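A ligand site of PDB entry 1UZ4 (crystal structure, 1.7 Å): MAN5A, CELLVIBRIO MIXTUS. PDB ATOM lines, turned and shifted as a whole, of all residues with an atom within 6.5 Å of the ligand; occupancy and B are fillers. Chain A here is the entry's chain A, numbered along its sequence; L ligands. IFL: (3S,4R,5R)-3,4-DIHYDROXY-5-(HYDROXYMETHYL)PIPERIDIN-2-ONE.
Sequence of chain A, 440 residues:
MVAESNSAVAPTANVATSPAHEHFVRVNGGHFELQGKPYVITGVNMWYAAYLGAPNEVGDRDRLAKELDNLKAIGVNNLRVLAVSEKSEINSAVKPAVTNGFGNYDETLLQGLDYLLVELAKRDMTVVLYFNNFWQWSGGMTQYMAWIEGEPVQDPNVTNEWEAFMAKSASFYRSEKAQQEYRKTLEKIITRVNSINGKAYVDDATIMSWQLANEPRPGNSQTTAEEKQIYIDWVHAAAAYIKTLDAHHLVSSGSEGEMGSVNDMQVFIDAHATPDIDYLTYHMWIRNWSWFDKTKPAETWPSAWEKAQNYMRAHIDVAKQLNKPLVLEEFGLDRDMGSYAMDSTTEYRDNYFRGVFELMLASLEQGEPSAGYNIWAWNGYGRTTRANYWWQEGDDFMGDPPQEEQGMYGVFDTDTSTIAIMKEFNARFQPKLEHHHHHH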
ATOM      1  N   ARG A  80       4.022 -17.879 -13.925  1.00  0.00           N
ATOM      2  CA  ARG A  80       3.446 -17.888 -12.584  1.00  0.00           C
ATOM      3  C   ARG A  80       3.132 -16.405 -12.224  1.00  0.00           C
ATOM      4  O   ARG A  80       4.017 -15.532 -12.266  1.00  0.00           O
ATOM      5  CB  ARG A  80       4.435 -18.522 -11.630  1.00  0.00           C
ATOM      6  CG  ARG A  80       3.993 -18.571 -10.170  1.00  0.00           C
ATOM      7  CD  ARG A  80       4.745 -19.512  -9.297  1.00  0.00           C
ATOM      8  NE  ARG A  80       4.296 -19.464  -7.909  1.00  0.00           N
ATOM      9  CZ  ARG A  80       4.776 -18.632  -6.998  1.00  0.00           C
ATOM     10  NH1 ARG A  80       5.750 -17.803  -7.309  1.00  0.00           N
ATOM     11  NH2 ARG A  80       4.336 -18.684  -5.759  1.00  0.00           N
ATOM     12  N   TYR A 130      -1.717 -17.476  -8.283  1.00  0.00           N
ATOM     13  CA  TYR A 130      -1.784 -17.543  -6.818  1.00  0.00           C
ATOM     14  C   TYR A 130      -2.655 -16.439  -6.216  1.00  0.00           C
ATOM     15  O   TYR A 130      -2.677 -15.319  -6.740  1.00  0.00           O
ATOM     16  CB  TYR A 130      -0.392 -17.561  -6.167  1.00  0.00           C
ATOM     17  CG  TYR A 130       0.619 -16.516  -6.616  1.00  0.00           C
ATOM     18  CD1 TYR A 130       0.816 -15.360  -5.916  1.00  0.00           C
ATOM     19  CD2 TYR A 130       1.424 -16.754  -7.743  1.00  0.00           C
ATOM     20  CE1 TYR A 130       1.799 -14.450  -6.280  1.00  0.00           C
ATOM     21  CE2 TYR A 130       2.402 -15.853  -8.117  1.00  0.00           C
ATOM     22  CZ  TYR A 130       2.577 -14.698  -7.414  1.00  0.00           C
ATOM     23  OH  TYR A 130       3.544 -13.817  -7.816  1.00  0.00           O
ATOM     24  N   ASN A 133      -0.712 -13.931  -0.496  1.00  0.00           N
ATOM     25  CA  ASN A 133       0.702 -13.673  -0.334  1.00  0.00           C
ATOM     26  C   ASN A 133       1.028 -13.666   1.132  1.00  0.00           C
ATOM     27  O   ASN A 133       0.406 -12.930   1.899  1.00  0.00           O
ATOM     28  CB  ASN A 133       1.071 -12.334  -0.960  1.00  0.00           C
ATOM     29  CG  ASN A 133       2.576 -12.190  -1.318  1.00  0.00           C
ATOM     30  OD1 ASN A 133       3.433 -12.960  -0.841  1.00  0.00           O
ATOM     31  ND2 ASN A 133       2.893 -11.166  -2.123  1.00  0.00           N
ATOM     32  N   TRP A 135       3.747 -12.488   2.094  1.00  0.00           N
ATOM     33  CA  TRP A 135       4.581 -11.280   2.200  1.00  0.00           C
ATOM     34  C   TRP A 135       3.782 -10.011   1.918  1.00  0.00           C
ATOM     35  O   TRP A 135       2.592 -10.078   1.630  1.00  0.00           O
ATOM     36  CB  TRP A 135       5.820 -11.393   1.300  1.00  0.00           C
ATOM     37  CG  TRP A 135       6.608 -12.668   1.594  1.00  0.00           C
ATOM     38  CD1 TRP A 135       6.766 -13.733   0.767  1.00  0.00           C
ATOM     39  CD2 TRP A 135       7.256 -13.031   2.826  1.00  0.00           C
ATOM     40  NE1 TRP A 135       7.483 -14.728   1.383  1.00  0.00           N
ATOM     41  CE2 TRP A 135       7.789 -14.323   2.662  1.00  0.00           C
ATOM     42  CE3 TRP A 135       7.454 -12.386   4.059  1.00  0.00           C
ATOM     43  CZ2 TRP A 135       8.507 -14.959   3.642  1.00  0.00           C
ATOM     44  CZ3 TRP A 135       8.172 -13.022   5.039  1.00  0.00           C
ATOM     45  CH2 TRP A 135       8.686 -14.298   4.836  1.00  0.00           C
ATOM     46  N   TRP A 137       4.086  -7.420  -0.387  1.00  0.00           N
ATOM     47  CA  TRP A 137       4.209  -6.634  -1.620  1.00  0.00           C
ATOM     48  C   TRP A 137       2.943  -6.593  -2.445  1.00  0.00           C
ATOM     49  O   TRP A 137       2.842  -5.825  -3.396  1.00  0.00           O
ATOM     50  CB  TRP A 137       5.410  -7.076  -2.459  1.00  0.00           C
ATOM     51  CG  TRP A 137       5.557  -8.542  -2.804  1.00  0.00           C
ATOM     52  CD1 TRP A 137       6.279  -9.483  -2.149  1.00  0.00           C
ATOM     53  CD2 TRP A 137       4.995  -9.212  -3.952  1.00  0.00           C
ATOM     54  NE1 TRP A 137       6.194 -10.694  -2.789  1.00  0.00           N
ATOM     55  CE2 TRP A 137       5.438 -10.551  -3.916  1.00  0.00           C
ATOM     56  CE3 TRP A 137       4.164  -8.803  -4.997  1.00  0.00           C
ATOM     57  CZ2 TRP A 137       5.074 -11.480  -4.896  1.00  0.00           C
ATOM     58  CZ3 TRP A 137       3.819  -9.739  -5.969  1.00  0.00           C
ATOM     59  CH2 TRP A 137       4.273 -11.059  -5.894  1.00  0.00           C
ATOM     60  N   ASN A 214       1.294 -17.163  -2.397  1.00  0.00           N
ATOM     61  CA  ASN A 214       2.738 -17.078  -2.536  1.00  0.00           C
ATOM     62  C   ASN A 214       3.440 -17.315  -1.192  1.00  0.00           C
ATOM     63  O   ASN A 214       3.288 -16.508  -0.270  1.00  0.00           O
ATOM     64  CB  ASN A 214       3.152 -15.731  -3.066  1.00  0.00           C
ATOM     65  CG  ASN A 214       4.643 -15.663  -3.340  1.00  0.00           C
ATOM     66  OD1 ASN A 214       5.207 -16.561  -3.968  1.00  0.00           O
ATOM     67  ND2 ASN A 214       5.285 -14.669  -2.749  1.00  0.00           N
ATOM     68  N   GLU A 215       4.133 -18.441  -1.083  1.00  0.00           N
ATOM     69  CA  GLU A 215       5.009 -18.765   0.046  1.00  0.00           C
ATOM     70  C   GLU A 215       4.295 -18.792   1.401  1.00  0.00           C
ATOM     71  O   GLU A 215       4.802 -18.263   2.366  1.00  0.00           O
ATOM     72  CB  GLU A 215       6.238 -17.840   0.060  1.00  0.00           C
ATOM     73  CG  GLU A 215       7.052 -17.980  -1.200  1.00  0.00           C
ATOM     74  CD  GLU A 215       8.473 -17.436  -1.116  1.00  0.00           C
ATOM     75  OE1 GLU A 215       8.724 -16.573  -0.223  1.00  0.00           O
ATOM     76  OE2 GLU A 215       9.328 -17.872  -1.942  1.00  0.00           O
ATOM     77  N   GLU A 256       7.436 -22.845  -0.330  1.00  0.00           N
ATOM     78  CA  GLU A 256       8.859 -22.858  -0.616  1.00  0.00           C
ATOM     79  C   GLU A 256       9.487 -24.233  -0.406  1.00  0.00           C
ATOM     80  O   GLU A 256      10.644 -24.441  -0.763  1.00  0.00           O
ATOM     81  CB  GLU A 256       9.595 -21.885   0.288  1.00  0.00           C
ATOM     82  CG  GLU A 256       9.159 -20.452   0.239  1.00  0.00           C
ATOM     83  CD  GLU A 256       9.457 -19.799   1.573  1.00  0.00           C
ATOM     84  OE1 GLU A 256       8.516 -19.687   2.384  1.00  0.00           O
ATOM     85  OE2 GLU A 256      10.667 -19.494   1.803  1.00  0.00           O
ATOM     86  N   HIS A 283      10.848 -23.603  -3.593  1.00  0.00           N
ATOM     87  CA  HIS A 283      11.489 -22.379  -4.032  1.00  0.00           C
ATOM     88  C   HIS A 283      12.888 -22.438  -3.470  1.00  0.00           C
ATOM     89  O   HIS A 283      13.066 -22.957  -2.361  1.00  0.00           O
ATOM     90  CB  HIS A 283      10.790 -21.145  -3.479  1.00  0.00           C
ATOM     91  CG  HIS A 283       9.351 -20.991  -3.837  1.00  0.00           C
ATOM     92  ND1 HIS A 283       8.627 -19.886  -3.440  1.00  0.00           N
ATOM     93  CD2 HIS A 283       8.493 -21.749  -4.564  1.00  0.00           C
ATOM     94  CE1 HIS A 283       7.376 -19.991  -3.871  1.00  0.00           C
ATOM     95  NE2 HIS A 283       7.275 -21.101  -4.572  1.00  0.00           N
ATOM     96  N   TRP A 285      16.303 -19.982  -2.582  1.00  0.00           N
ATOM     97  CA  TRP A 285      16.786 -18.620  -2.395  1.00  0.00           C
ATOM     98  C   TRP A 285      18.110 -18.568  -1.608  1.00  0.00           C
ATOM     99  O   TRP A 285      18.148 -18.207  -0.434  1.00  0.00           O
ATOM    100  CB  TRP A 285      15.699 -17.748  -1.747  1.00  0.00           C
ATOM    101  CG  TRP A 285      14.594 -17.525  -2.752  1.00  0.00           C
ATOM    102  CD1 TRP A 285      13.328 -18.009  -2.732  1.00  0.00           C
ATOM    103  CD2 TRP A 285      14.742 -16.791  -3.937  1.00  0.00           C
ATOM    104  NE1 TRP A 285      12.664 -17.601  -3.863  1.00  0.00           N
ATOM    105  CE2 TRP A 285      13.531 -16.875  -4.644  1.00  0.00           C
ATOM    106  CE3 TRP A 285      15.801 -16.068  -4.505  1.00  0.00           C
ATOM    107  CZ2 TRP A 285      13.326 -16.220  -5.854  1.00  0.00           C
ATOM    108  CZ3 TRP A 285      15.617 -15.435  -5.747  1.00  0.00           C
ATOM    109  CH2 TRP A 285      14.372 -15.511  -6.390  1.00  0.00           C
ATOM    110  N   ARG A 287      20.771 -16.718  -1.629  1.00  0.00           N
ATOM    111  CA  ARG A 287      21.274 -15.468  -1.020  1.00  0.00           C
ATOM    112  C   ARG A 287      20.362 -15.084   0.164  1.00  0.00           C
ATOM    113  O   ARG A 287      20.850 -14.724   1.245  1.00  0.00           O
ATOM    114  CB  ARG A 287      21.397 -14.343  -2.040  1.00  0.00           C
ATOM    115  CG  ARG A 287      22.167 -13.137  -1.526  1.00  0.00           C
ATOM    116  CD  ARG A 287      21.276 -12.141  -0.869  1.00  0.00           C
ATOM    117  NE  ARG A 287      20.579 -11.420  -1.923  1.00  0.00           N
ATOM    118  CZ  ARG A 287      19.399 -10.835  -1.803  1.00  0.00           C
ATOM    119  NH1 ARG A 287      18.882 -10.201  -2.853  1.00  0.00           N
ATOM    120  NH2 ARG A 287      18.714 -10.877  -0.672  1.00  0.00           N
ATOM    121  N   ASN A 288      19.043 -15.144  -0.011  1.00  0.00           N
ATOM    122  CA  ASN A 288      18.097 -14.764   1.056  1.00  0.00           C
ATOM    123  C   ASN A 288      18.346 -15.585   2.336  1.00  0.00           C
ATOM    124  O   ASN A 288      18.151 -15.096   3.459  1.00  0.00           O
ATOM    125  CB  ASN A 288      16.651 -15.023   0.647  1.00  0.00           C
ATOM    126  CG  ASN A 288      16.219 -14.231  -0.595  1.00  0.00           C
ATOM    127  OD1 ASN A 288      17.014 -14.026  -1.509  1.00  0.00           O
ATOM    128  ND2 ASN A 288      14.947 -13.878  -0.642  1.00  0.00           N
ATOM    129  N   GLU A 330      10.135 -21.169  -8.048  1.00  0.00           N
ATOM    130  CA  GLU A 330      10.934 -19.945  -7.929  1.00  0.00           C
ATOM    131  C   GLU A 330      12.376 -20.310  -7.616  1.00  0.00           C
ATOM    132  O   GLU A 330      12.649 -21.123  -6.731  1.00  0.00           O
ATOM    133  CB  GLU A 330      10.514 -19.021  -6.773  1.00  0.00           C
ATOM    134  CG  GLU A 330       9.117 -18.499  -6.701  1.00  0.00           C
ATOM    135  CD  GLU A 330       8.964 -17.483  -5.572  1.00  0.00           C
ATOM    136  OE1 GLU A 330       7.830 -17.019  -5.323  1.00  0.00           O
ATOM    137  OE2 GLU A 330       9.978 -17.126  -4.963  1.00  0.00           O
ATOM    138  N   TRP A 376      12.789 -17.007 -11.202  1.00  0.00           N
ATOM    139  CA  TRP A 376      12.395 -15.735 -10.598  1.00  0.00           C
ATOM    140  C   TRP A 376      13.523 -14.753 -10.897  1.00  0.00           C
ATOM    141  O   TRP A 376      14.621 -14.902 -10.335  1.00  0.00           O
ATOM    142  CB  TRP A 376      12.193 -15.849  -9.069  1.00  0.00           C
ATOM    143  CG  TRP A 376      11.695 -14.581  -8.516  1.00  0.00           C
ATOM    144  CD1 TRP A 376      12.410 -13.422  -8.277  1.00  0.00           C
ATOM    145  CD2 TRP A 376      10.337 -14.285  -8.132  1.00  0.00           C
ATOM    146  NE1 TRP A 376      11.581 -12.452  -7.786  1.00  0.00           N
ATOM    147  CE2 TRP A 376      10.305 -12.949  -7.695  1.00  0.00           C
ATOM    148  CE3 TRP A 376       9.147 -15.028  -8.093  1.00  0.00           C
ATOM    149  CZ2 TRP A 376       9.136 -12.359  -7.224  1.00  0.00           C
ATOM    150  CZ3 TRP A 376       7.983 -14.420  -7.653  1.00  0.00           C
ATOM    151  CH2 TRP A 376       7.988 -13.100  -7.220  1.00  0.00           C
ATOM    152  N   GLY A 399       9.826  -7.980 -12.838  1.00  0.00           N
ATOM    153  CA  GLY A 399       9.767  -9.250 -12.132  1.00  0.00           C
ATOM    154  C   GLY A 399      10.112  -9.122 -10.671  1.00  0.00           C
ATOM    155  O   GLY A 399       9.597  -9.852  -9.823  1.00  0.00           O
ATOM    156  N   ASP A 400      10.969  -8.151 -10.381  1.00  0.00           N
ATOM    157  CA  ASP A 400      11.238  -7.724  -9.009  1.00  0.00           C
ATOM    158  C   ASP A 400       9.998  -6.972  -8.525  1.00  0.00           C
ATOM    159  O   ASP A 400       9.660  -5.962  -9.127  1.00  0.00           O
ATOM    160  CB  ASP A 400      12.432  -6.797  -9.042  1.00  0.00           C
ATOM    161  CG  ASP A 400      13.696  -7.494  -9.519  1.00  0.00           C
ATOM    162  OD1 ASP A 400      14.106  -8.431  -8.825  1.00  0.00           O
ATOM    163  OD2 ASP A 400      14.357  -7.174 -10.543  1.00  0.00           O
ATOM    164  N   PRO A 401       9.273  -7.417  -7.502  1.00  0.00           N
ATOM    165  CA  PRO A 401       8.078  -6.676  -7.072  1.00  0.00           C
ATOM    166  C   PRO A 401       8.435  -5.427  -6.248  1.00  0.00           C
ATOM    167  O   PRO A 401       9.623  -5.169  -6.045  1.00  0.00           O
ATOM    168  CB  PRO A 401       7.264  -7.685  -6.280  1.00  0.00           C
ATOM    169  CG  PRO A 401       7.994  -8.997  -6.463  1.00  0.00           C
ATOM    170  CD  PRO A 401       9.472  -8.615  -6.682  1.00  0.00           C
ATOM    171  N   GLN A 403       8.698  -4.466  -3.309  1.00  0.00           N
ATOM    172  CA  GLN A 403       9.392  -4.552  -2.038  1.00  0.00           C
ATOM    173  C   GLN A 403      10.899  -4.800  -2.196  1.00  0.00           C
ATOM    174  O   GLN A 403      11.635  -4.888  -1.209  1.00  0.00           O
ATOM    175  CB  GLN A 403       8.743  -5.635  -1.129  1.00  0.00           C
ATOM    176  CG  GLN A 403       9.305  -7.040  -1.153  1.00  0.00           C
ATOM    177  CD  GLN A 403       9.217  -7.769  -2.465  1.00  0.00           C
ATOM    178  OE1 GLN A 403       8.722  -7.226  -3.435  1.00  0.00           O
ATOM    179  NE2 GLN A 403       9.670  -9.050  -2.472  1.00  0.00           N
ATOM    180  N   GLU A 404      11.378  -4.937  -3.434  1.00  0.00           N
ATOM    181  CA  GLU A 404      12.774  -5.158  -3.743  1.00  0.00           C
ATOM    182  C   GLU A 404      13.240  -4.192  -4.803  1.00  0.00           C
ATOM    183  O   GLU A 404      12.478  -3.758  -5.674  1.00  0.00           O
ATOM    184  CB  GLU A 404      13.024  -6.628  -4.148  1.00  0.00           C
ATOM    185  CG  GLU A 404      13.042  -7.540  -2.935  1.00  0.00           C
ATOM    186  CD  GLU A 404      12.978  -9.031  -3.209  1.00  0.00           C
ATOM    187  OE1 GLU A 404      12.656  -9.476  -4.345  1.00  0.00           O
ATOM    188  OE2 GLU A 404      13.229  -9.763  -2.213  1.00  0.00           O
ATOM    189  N   MET A 408      17.078  -6.433  -8.889  1.00  0.00           N
ATOM    190  CA  MET A 408      17.675  -7.391  -7.961  1.00  0.00           C
ATOM    191  C   MET A 408      17.866  -8.804  -8.562  1.00  0.00           C
ATOM    192  O   MET A 408      18.994  -9.311  -8.659  1.00  0.00           O
ATOM    193  CB  MET A 408      16.876  -7.451  -6.668  1.00  0.00           C
ATOM    194  CG  MET A 408      17.461  -8.368  -5.690  1.00  0.00           C
ATOM    195  SD  MET A 408      16.532  -8.378  -4.124  1.00  0.00           S
ATOM    196  CE  MET A 408      17.057  -6.862  -3.452  1.00  0.00           C
ATOM    197  N   TYR A 409      16.768  -9.397  -8.978  1.00  0.00           N
ATOM    198  CA  TYR A 409      16.738 -10.764  -9.469  1.00  0.00           C
ATOM    199  C   TYR A 409      16.229 -10.897 -10.904  1.00  0.00           C
ATOM    200  O   TYR A 409      16.378 -11.955 -11.499  1.00  0.00           O
ATOM    201  CB  TYR A 409      15.872 -11.613  -8.564  1.00  0.00           C
ATOM    202  CG  TYR A 409      16.493 -11.936  -7.220  1.00  0.00           C
ATOM    203  CD1 TYR A 409      17.749 -12.509  -7.147  1.00  0.00           C
ATOM    204  CD2 TYR A 409      15.789 -11.773  -6.062  1.00  0.00           C
ATOM    205  CE1 TYR A 409      18.316 -12.881  -5.927  1.00  0.00           C
ATOM    206  CE2 TYR A 409      16.339 -12.137  -4.830  1.00  0.00           C
ATOM    207  CZ  TYR A 409      17.592 -12.688  -4.777  1.00  0.00           C
ATOM    208  OH  TYR A 409      18.129 -13.126  -3.583  1.00  0.00           O
HETATM  209  O4  IFL L   1      10.543 -11.266  -4.337  1.00  0.00           O
HETATM  210  C4  IFL L   1      10.576 -12.357  -3.453  1.00  0.00           C
HETATM  211  C3  IFL L   1       9.141 -12.977  -3.454  1.00  0.00           C
HETATM  212  O3  IFL L   1       8.387 -12.468  -2.328  1.00  0.00           O
HETATM  213  C2  IFL L   1       9.080 -14.520  -3.295  1.00  0.00           C
HETATM  214  N   IFL L   1      10.190 -15.127  -2.845  1.00  0.00           N
HETATM  215  C7  IFL L   1      11.521 -14.504  -2.804  1.00  0.00           C
HETATM  216  C5  IFL L   1      11.653 -13.382  -3.835  1.00  0.00           C
HETATM  217  C6  IFL L   1      13.126 -12.891  -3.895  1.00  0.00           C
HETATM  218  O6  IFL L   1      13.506 -12.342  -2.607  1.00  0.00           O
HETATM  219  O2  IFL L   1       7.976 -15.090  -3.379  1.00  0.00           O
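The side-chain carboxylate (OE1) of Glu 330 is in salt-bridge range of the guanidinium group (NH1) of Arg 80 (3.0 Å). The side-chain amide nitrogen of Asn 214 is in hydrogen-bond range of the side-chain amide oxygen of Asn 133 (3.2 Å). NE1 of Trp 137 sits close to ND2 of Asn 133, 3.4 Å away. OD1 of Asn 288 is in hydrogen-bond range of OH of Tyr 409, at 2.5 Å. The side-chain carboxylate (OE1) of Glu 215 lies within hydrogen-bond range of the indole nitrogen (NE1) of Trp 135 (2.7 Å). OE1 of Gln 403 sits close to O of Pro 401 (3.4 Å). The side-chain hydroxyl (OH) of Tyr 409 lies within hydrogen-bond range of the guanidinium group (NH1) of Arg 287, at 3.1 Å. N of Trp 135 sits at hydrogen-bond distance from OD1 of Asn 133 (3.0 Å).
CD1 of Trp 135 touches O3 of the ligand, at 3.7 Å. NE1 of Trp 285 touches C7 of the ligand, 3.5 Å away. Trp 376 touches the ligand. Pro 401 touches the ligand. Tyr 409 touches the ligand. Hydrophobic or aromatic side chains that line the ligand: Trp 135, Trp 137, Trp 285, Trp 376, Pro 401 and Tyr 409.
O6 of the ligand is in hydrogen-bond range of OE2 of Glu 404, at 2.6 Å. OE2 of Glu 330 is in hydrogen-bond range of N of the ligand. O2 of the ligand sits at hydrogen-bond distance from ND2 of Asn 214 (2.8 Å). O3 of the ligand sits at hydrogen-bond distance from NE1 of Trp 137 (2.9 Å). O6 of the ligand is in hydrogen-bond range of ND2 of Asn 288, 2.9 Å away. N of the ligand lies within hydrogen-bond range of OE2 of Glu 215 (3.0 Å). NE2 of Gln 403 lies within hydrogen-bond range of O4 of the ligand, 3.0 Å away.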
